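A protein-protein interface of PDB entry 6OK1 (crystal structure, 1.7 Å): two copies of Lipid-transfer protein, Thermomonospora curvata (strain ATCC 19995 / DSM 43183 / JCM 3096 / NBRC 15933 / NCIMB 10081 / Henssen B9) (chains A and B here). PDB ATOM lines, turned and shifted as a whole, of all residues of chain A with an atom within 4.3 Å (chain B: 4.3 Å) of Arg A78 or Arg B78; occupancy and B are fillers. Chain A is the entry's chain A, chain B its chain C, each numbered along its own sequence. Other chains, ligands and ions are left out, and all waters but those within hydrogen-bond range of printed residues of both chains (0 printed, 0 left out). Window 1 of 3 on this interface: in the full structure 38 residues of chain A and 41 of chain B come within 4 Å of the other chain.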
ATOM      1  N   THR A  53      24.528  -9.056 -28.477  1.00  0.00           N
ATOM      2  CA  THR A  53      23.890  -8.950 -29.794  1.00  0.00           C
ATOM      3  C   THR A  53      22.873 -10.079 -29.934  1.00  0.00           C
ATOM      4  O   THR A  53      22.504 -10.738 -28.954  1.00  0.00           O
ATOM      5  CB  THR A  53      24.936  -8.909 -30.921  1.00  0.00           C
ATOM      6  OG1 THR A  53      24.295  -8.667 -32.174  1.00  0.00           O
ATOM      7  CG2 THR A  53      25.729 -10.188 -31.023  1.00  0.00           C
ATOM      8  N   PHE A  54      22.368 -10.250 -31.151  1.00  0.00           N
ATOM      9  CA  PHE A  54      21.389 -11.274 -31.485  1.00  0.00           C
ATOM     10  C   PHE A  54      22.090 -12.593 -31.807  1.00  0.00           C
ATOM     11  O   PHE A  54      23.215 -12.608 -32.309  1.00  0.00           O
ATOM     12  CB  PHE A  54      20.579 -10.882 -32.725  1.00  0.00           C
ATOM     13  CG  PHE A  54      19.643  -9.676 -32.569  1.00  0.00           C
ATOM     14  CD1 PHE A  54      19.851  -8.648 -31.626  1.00  0.00           C
ATOM     15  CD2 PHE A  54      18.570  -9.564 -33.451  1.00  0.00           C
ATOM     16  CE1 PHE A  54      18.991  -7.550 -31.583  1.00  0.00           C
ATOM     17  CE2 PHE A  54      17.699  -8.455 -33.397  1.00  0.00           C
ATOM     18  CZ  PHE A  54      17.901  -7.483 -32.460  1.00  0.00           C
ATOM     19  N   THR A  55      21.371 -13.704 -31.632  1.00  0.00           N
ATOM     20  CA  THR A  55      21.980 -15.000 -31.970  1.00  0.00           C
ATOM     21  C   THR A  55      22.452 -15.039 -33.424  1.00  0.00           C
ATOM     22  O   THR A  55      23.516 -15.608 -33.726  1.00  0.00           O
ATOM     23  CB  THR A  55      21.005 -16.152 -31.694  1.00  0.00           C
ATOM     24  OG1 THR A  55      19.716 -15.836 -32.229  1.00  0.00           O
ATOM     25  CG2 THR A  55      20.840 -16.337 -30.257  1.00  0.00           C
ATOM     26  N   ASP A  57      23.429 -12.592 -35.433  1.00  0.00           N
ATOM     27  CA  ASP A  57      24.414 -11.619 -35.858  1.00  0.00           C
ATOM     28  C   ASP A  57      25.751 -12.304 -36.121  1.00  0.00           C
ATOM     29  O   ASP A  57      26.235 -13.074 -35.288  1.00  0.00           O
ATOM     30  CB  ASP A  57      24.565 -10.517 -34.821  1.00  0.00           C
ATOM     31  CG  ASP A  57      25.197  -9.286 -35.425  1.00  0.00           C
ATOM     32  OD1 ASP A  57      26.418  -9.327 -35.674  1.00  0.00           O
ATOM     33  OD2 ASP A  57      24.489  -8.296 -35.728  1.00  0.00           O
ATOM     34  N   SER A  60      30.669 -11.551 -34.458  1.00  0.00           N
ATOM     35  CA  SER A  60      30.750 -11.987 -33.074  1.00  0.00           C
ATOM     36  C   SER A  60      31.412 -10.929 -32.189  1.00  0.00           C
ATOM     37  O   SER A  60      32.192 -10.081 -32.642  1.00  0.00           O
ATOM     38  CB  SER A  60      31.512 -13.308 -32.990  1.00  0.00           C
ATOM     39  OG  SER A  60      32.888 -13.045 -33.060  1.00  0.00           O
ATOM     40  N   GLU A  61      31.145 -11.052 -30.881  1.00  0.00           N
ATOM     41  CA  GLU A  61      31.693 -10.133 -29.899  1.00  0.00           C
ATOM     42  C   GLU A  61      33.206 -10.039 -30.030  1.00  0.00           C
ATOM     43  O   GLU A  61      33.773  -8.951 -29.926  1.00  0.00           O
ATOM     44  CB  GLU A  61      31.314 -10.591 -28.479  1.00  0.00           C
ATOM     45  CG  GLU A  61      29.796 -10.746 -28.271  1.00  0.00           C
ATOM     46  CD  GLU A  61      29.293 -12.144 -28.480  1.00  0.00           C
ATOM     47  OE1 GLU A  61      29.789 -12.838 -29.400  1.00  0.00           O
ATOM     48  OE2 GLU A  61      28.396 -12.556 -27.714  1.00  0.00           O
ATOM     49  N   SER A  77      26.829 -12.010 -24.490  1.00  0.00           N
ATOM     50  CA  SER A  77      25.631 -12.839 -24.487  1.00  0.00           C
ATOM     51  C   SER A  77      24.829 -12.543 -25.740  1.00  0.00           C
ATOM     52  O   SER A  77      25.031 -11.519 -26.412  1.00  0.00           O
ATOM     53  CB  SER A  77      24.759 -12.571 -23.250  1.00  0.00           C
ATOM     54  OG  SER A  77      24.226 -11.246 -23.311  1.00  0.00           O
ATOM     55  N   ARG A  78      23.895 -13.439 -26.014  1.00  0.00           N
ATOM     56  CA  ARG A  78      22.994 -13.315 -27.152  1.00  0.00           C
ATOM     57  C   ARG A  78      21.568 -13.536 -26.694  1.00  0.00           C
ATOM     58  O   ARG A  78      21.307 -14.249 -25.723  1.00  0.00           O
ATOM     59  CB  ARG A  78      23.275 -14.328 -28.249  1.00  0.00           C
ATOM     60  CG  ARG A  78      24.712 -14.370 -28.706  1.00  0.00           C
ATOM     61  CD  ARG A  78      25.157 -13.118 -29.384  1.00  0.00           C
ATOM     62  NE  ARG A  78      26.489 -13.332 -29.937  1.00  0.00           N
ATOM     63  CZ  ARG A  78      26.776 -13.618 -31.210  1.00  0.00           C
ATOM     64  NH1 ARG A  78      25.829 -13.702 -32.150  1.00  0.00           N
ATOM     65  NH2 ARG A  78      28.054 -13.766 -31.566  1.00  0.00           N
ATOM     66  N   VAL A  79      20.633 -12.938 -27.430  1.00  0.00           N
ATOM     67  CA  VAL A  79      19.217 -13.234 -27.276  1.00  0.00           C
ATOM     68  C   VAL A  79      18.691 -13.642 -28.641  1.00  0.00           C
ATOM     69  O   VAL A  79      19.099 -13.071 -29.659  1.00  0.00           O
ATOM     70  CB  VAL A  79      18.455 -12.022 -26.697  1.00  0.00           C
ATOM     71  CG1 VAL A  79      16.966 -12.345 -26.592  1.00  0.00           C
ATOM     72  CG2 VAL A  79      19.027 -11.646 -25.309  1.00  0.00           C
ATOM     73  N   THR B  53      20.653 -21.561 -22.680  1.00  0.00           N
ATOM     74  CA  THR B  53      21.429 -22.590 -23.351  1.00  0.00           C
ATOM     75  C   THR B  53      22.504 -21.931 -24.211  1.00  0.00           C
ATOM     76  O   THR B  53      22.791 -20.729 -24.088  1.00  0.00           O
ATOM     77  CB  THR B  53      20.507 -23.557 -24.124  1.00  0.00           C
ATOM     78  OG1 THR B  53      21.277 -24.664 -24.639  1.00  0.00           O
ATOM     79  CG2 THR B  53      19.799 -22.884 -25.292  1.00  0.00           C
ATOM     80  N   PHE B  54      23.161 -22.744 -25.024  1.00  0.00           N
ATOM     81  CA  PHE B  54      24.231 -22.311 -25.900  1.00  0.00           C
ATOM     82  C   PHE B  54      23.643 -21.836 -27.223  1.00  0.00           C
ATOM     83  O   PHE B  54      22.601 -22.324 -27.669  1.00  0.00           O
ATOM     84  CB  PHE B  54      25.203 -23.453 -26.219  1.00  0.00           C
ATOM     85  CG  PHE B  54      26.022 -24.006 -25.059  1.00  0.00           C
ATOM     86  CD1 PHE B  54      25.648 -23.936 -23.722  1.00  0.00           C
ATOM     87  CD2 PHE B  54      27.182 -24.712 -25.385  1.00  0.00           C
ATOM     88  CE1 PHE B  54      26.442 -24.533 -22.730  1.00  0.00           C
ATOM     89  CE2 PHE B  54      27.969 -25.326 -24.404  1.00  0.00           C
ATOM     90  CZ  PHE B  54      27.601 -25.234 -23.082  1.00  0.00           C
ATOM     91  N   THR B  55      24.370 -20.935 -27.892  1.00  0.00           N
ATOM     92  CA  THR B  55      23.900 -20.453 -29.197  1.00  0.00           C
ATOM     93  C   THR B  55      23.642 -21.604 -30.162  1.00  0.00           C
ATOM     94  O   THR B  55      22.667 -21.580 -30.924  1.00  0.00           O
ATOM     95  CB  THR B  55      24.899 -19.469 -29.803  1.00  0.00           C
ATOM     96  OG1 THR B  55      26.223 -20.008 -29.754  1.00  0.00           O
ATOM     97  CG2 THR B  55      24.900 -18.211 -29.024  1.00  0.00           C
ATOM     98  N   ASP B  57      22.774 -24.710 -29.552  1.00  0.00           N
ATOM     99  CA  ASP B  57      21.792 -25.729 -29.193  1.00  0.00           C
ATOM    100  C   ASP B  57      20.560 -25.582 -30.082  1.00  0.00           C
ATOM    101  O   ASP B  57      20.007 -24.485 -30.218  1.00  0.00           O
ATOM    102  CB  ASP B  57      21.420 -25.636 -27.709  1.00  0.00           C
ATOM    103  CG  ASP B  57      20.807 -26.926 -27.197  1.00  0.00           C
ATOM    104  OD1 ASP B  57      19.633 -27.184 -27.522  1.00  0.00           O
ATOM    105  OD2 ASP B  57      21.497 -27.730 -26.519  1.00  0.00           O
ATOM    106  N   SER B  60      15.409 -25.040 -29.050  1.00  0.00           N
ATOM    107  CA  SER B  60      15.224 -23.691 -28.558  1.00  0.00           C
ATOM    108  C   SER B  60      14.363 -23.694 -27.301  1.00  0.00           C
ATOM    109  O   SER B  60      13.584 -24.628 -27.030  1.00  0.00           O
ATOM    110  CB  SER B  60      14.579 -22.817 -29.631  1.00  0.00           C
ATOM    111  OG  SER B  60      13.220 -23.159 -29.677  1.00  0.00           O
ATOM    112  N   GLU B  61      14.463 -22.583 -26.568  1.00  0.00           N
ATOM    113  CA  GLU B  61      13.754 -22.434 -25.307  1.00  0.00           C
ATOM    114  C   GLU B  61      12.262 -22.683 -25.472  1.00  0.00           C
ATOM    115  O   GLU B  61      11.651 -23.345 -24.634  1.00  0.00           O
ATOM    116  CB  GLU B  61      14.011 -21.041 -24.732  1.00  0.00           C
ATOM    117  CG  GLU B  61      15.504 -20.728 -24.522  1.00  0.00           C
ATOM    118  CD  GLU B  61      16.114 -19.954 -25.676  1.00  0.00           C
ATOM    119  OE1 GLU B  61      15.752 -20.208 -26.850  1.00  0.00           O
ATOM    120  OE2 GLU B  61      16.956 -19.069 -25.405  1.00  0.00           O
ATOM    121  N   SER B  77      18.039 -16.728 -22.796  1.00  0.00           N
ATOM    122  CA  SER B  77      19.263 -16.157 -23.328  1.00  0.00           C
ATOM    123  C   SER B  77      20.186 -17.277 -23.776  1.00  0.00           C
ATOM    124  O   SER B  77      19.998 -18.446 -23.424  1.00  0.00           O
ATOM    125  CB  SER B  77      19.975 -15.292 -22.273  1.00  0.00           C
ATOM    126  OG  SER B  77      20.413 -16.096 -21.189  1.00  0.00           O
ATOM    127  N   ARG B  78      21.198 -16.894 -24.545  1.00  0.00           N
ATOM    128  CA  ARG B  78      22.226 -17.808 -25.027  1.00  0.00           C
ATOM    129  C   ARG B  78      23.595 -17.225 -24.735  1.00  0.00           C
ATOM    130  O   ARG B  78      23.774 -16.010 -24.645  1.00  0.00           O
ATOM    131  CB  ARG B  78      22.162 -18.081 -26.550  1.00  0.00           C
ATOM    132  CG  ARG B  78      20.794 -18.471 -27.084  1.00  0.00           C
ATOM    133  CD  ARG B  78      20.353 -19.770 -26.526  1.00  0.00           C
ATOM    134  NE  ARG B  78      19.113 -20.176 -27.192  1.00  0.00           N
ATOM    135  CZ  ARG B  78      19.014 -21.020 -28.222  1.00  0.00           C
ATOM    136  NH1 ARG B  78      20.072 -21.629 -28.747  1.00  0.00           N
ATOM    137  NH2 ARG B  78      17.818 -21.262 -28.742  1.00  0.00           N
ATOM    138  N   VAL B  79      24.571 -18.110 -24.648  1.00  0.00           N
ATOM    139  CA  VAL B  79      25.971 -17.725 -24.601  1.00  0.00           C
ATOM    140  C   VAL B  79      26.664 -18.522 -25.699  1.00  0.00           C
ATOM    141  O   VAL B  79      26.376 -19.714 -25.906  1.00  0.00           O
ATOM    142  CB  VAL B  79      26.611 -17.976 -23.211  1.00  0.00           C
ATOM    143  CG1 VAL B  79      28.103 -17.572 -23.205  1.00  0.00           C
ATOM    144  CG2 VAL B  79      25.861 -17.166 -22.096  1.00  0.00           C
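Thr A55 touches Arg B78, and with the chains exchanged Arg A78 touches Thr B55. Ser A77 touches Arg B78, and with the chains exchanged Arg A78 touches Ser B77. Arg A78 touches its own counterpart, Arg B78.
O of Phe A54 lies within hydrogen-bond range of NH1 of Arg A78, 2.8 Å away. The backbone NH (N) of Thr B53 is in hydrogen-bond range of the backbone carbonyl oxygen (O) of Ser B77. O of Phe B54 lies within hydrogen-bond range of NH1 of Arg B78. The backbone NH of Thr B55 sits at hydrogen-bond distance from the backbone carbonyl oxygen of Val B79 (3.1 Å). The backbone carbonyl oxygen (O) of Asp B57 sits at hydrogen-bond distance from the guanidinium group (NH1) of Arg B78. The guanidinium group (NH2) of Arg B78 lies within salt-bridge range of the side-chain carboxylate (OE1) of Glu B61, 3.0 Å away.
Along chain B the printed residues that touch a printed residue of chain A span positions 55 to 78. Of the 9 printed residues of chain A, 3 touch a printed residue of chain B.
Of chain B, only Thr B55 (3.9 Å), Ser B77 (3.7 Å) and Arg B78 (2.9 Å) come within 4 Å of Arg A78. Arg B78 touches just these residues of chain A: Thr A55, Ser A77 and Arg A78. Of the printed residues of chain A, Ser B77 touches Arg A78. Of the printed residues of chain B, Thr A55 touches Arg B78. Printed residues of chain A within 4 Å of Thr B55: Arg A78. Printed residues of chain B within 4 Å of Ser A77: Arg B78 (3.7 Å). Val A79 touches none of the printed residues of chain B. The nearest printed residue of chain B that does not touch Arg A78 is Val B79 (4.9 Å).
The backbone carbonyl oxygen of Arg A78 lies within hydrogen-bond range of the backbone NH of Arg B78, 2.9 Å away.
Among the printed residues, merely in contact across the chains: Ser A77 with Arg B78 (3.7 Å), Arg A78 with Ser B77 (3.7 Å), Thr A55 with Arg B78 (3.8 Å) and Arg A78 with Thr B55 (3.9 Å).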
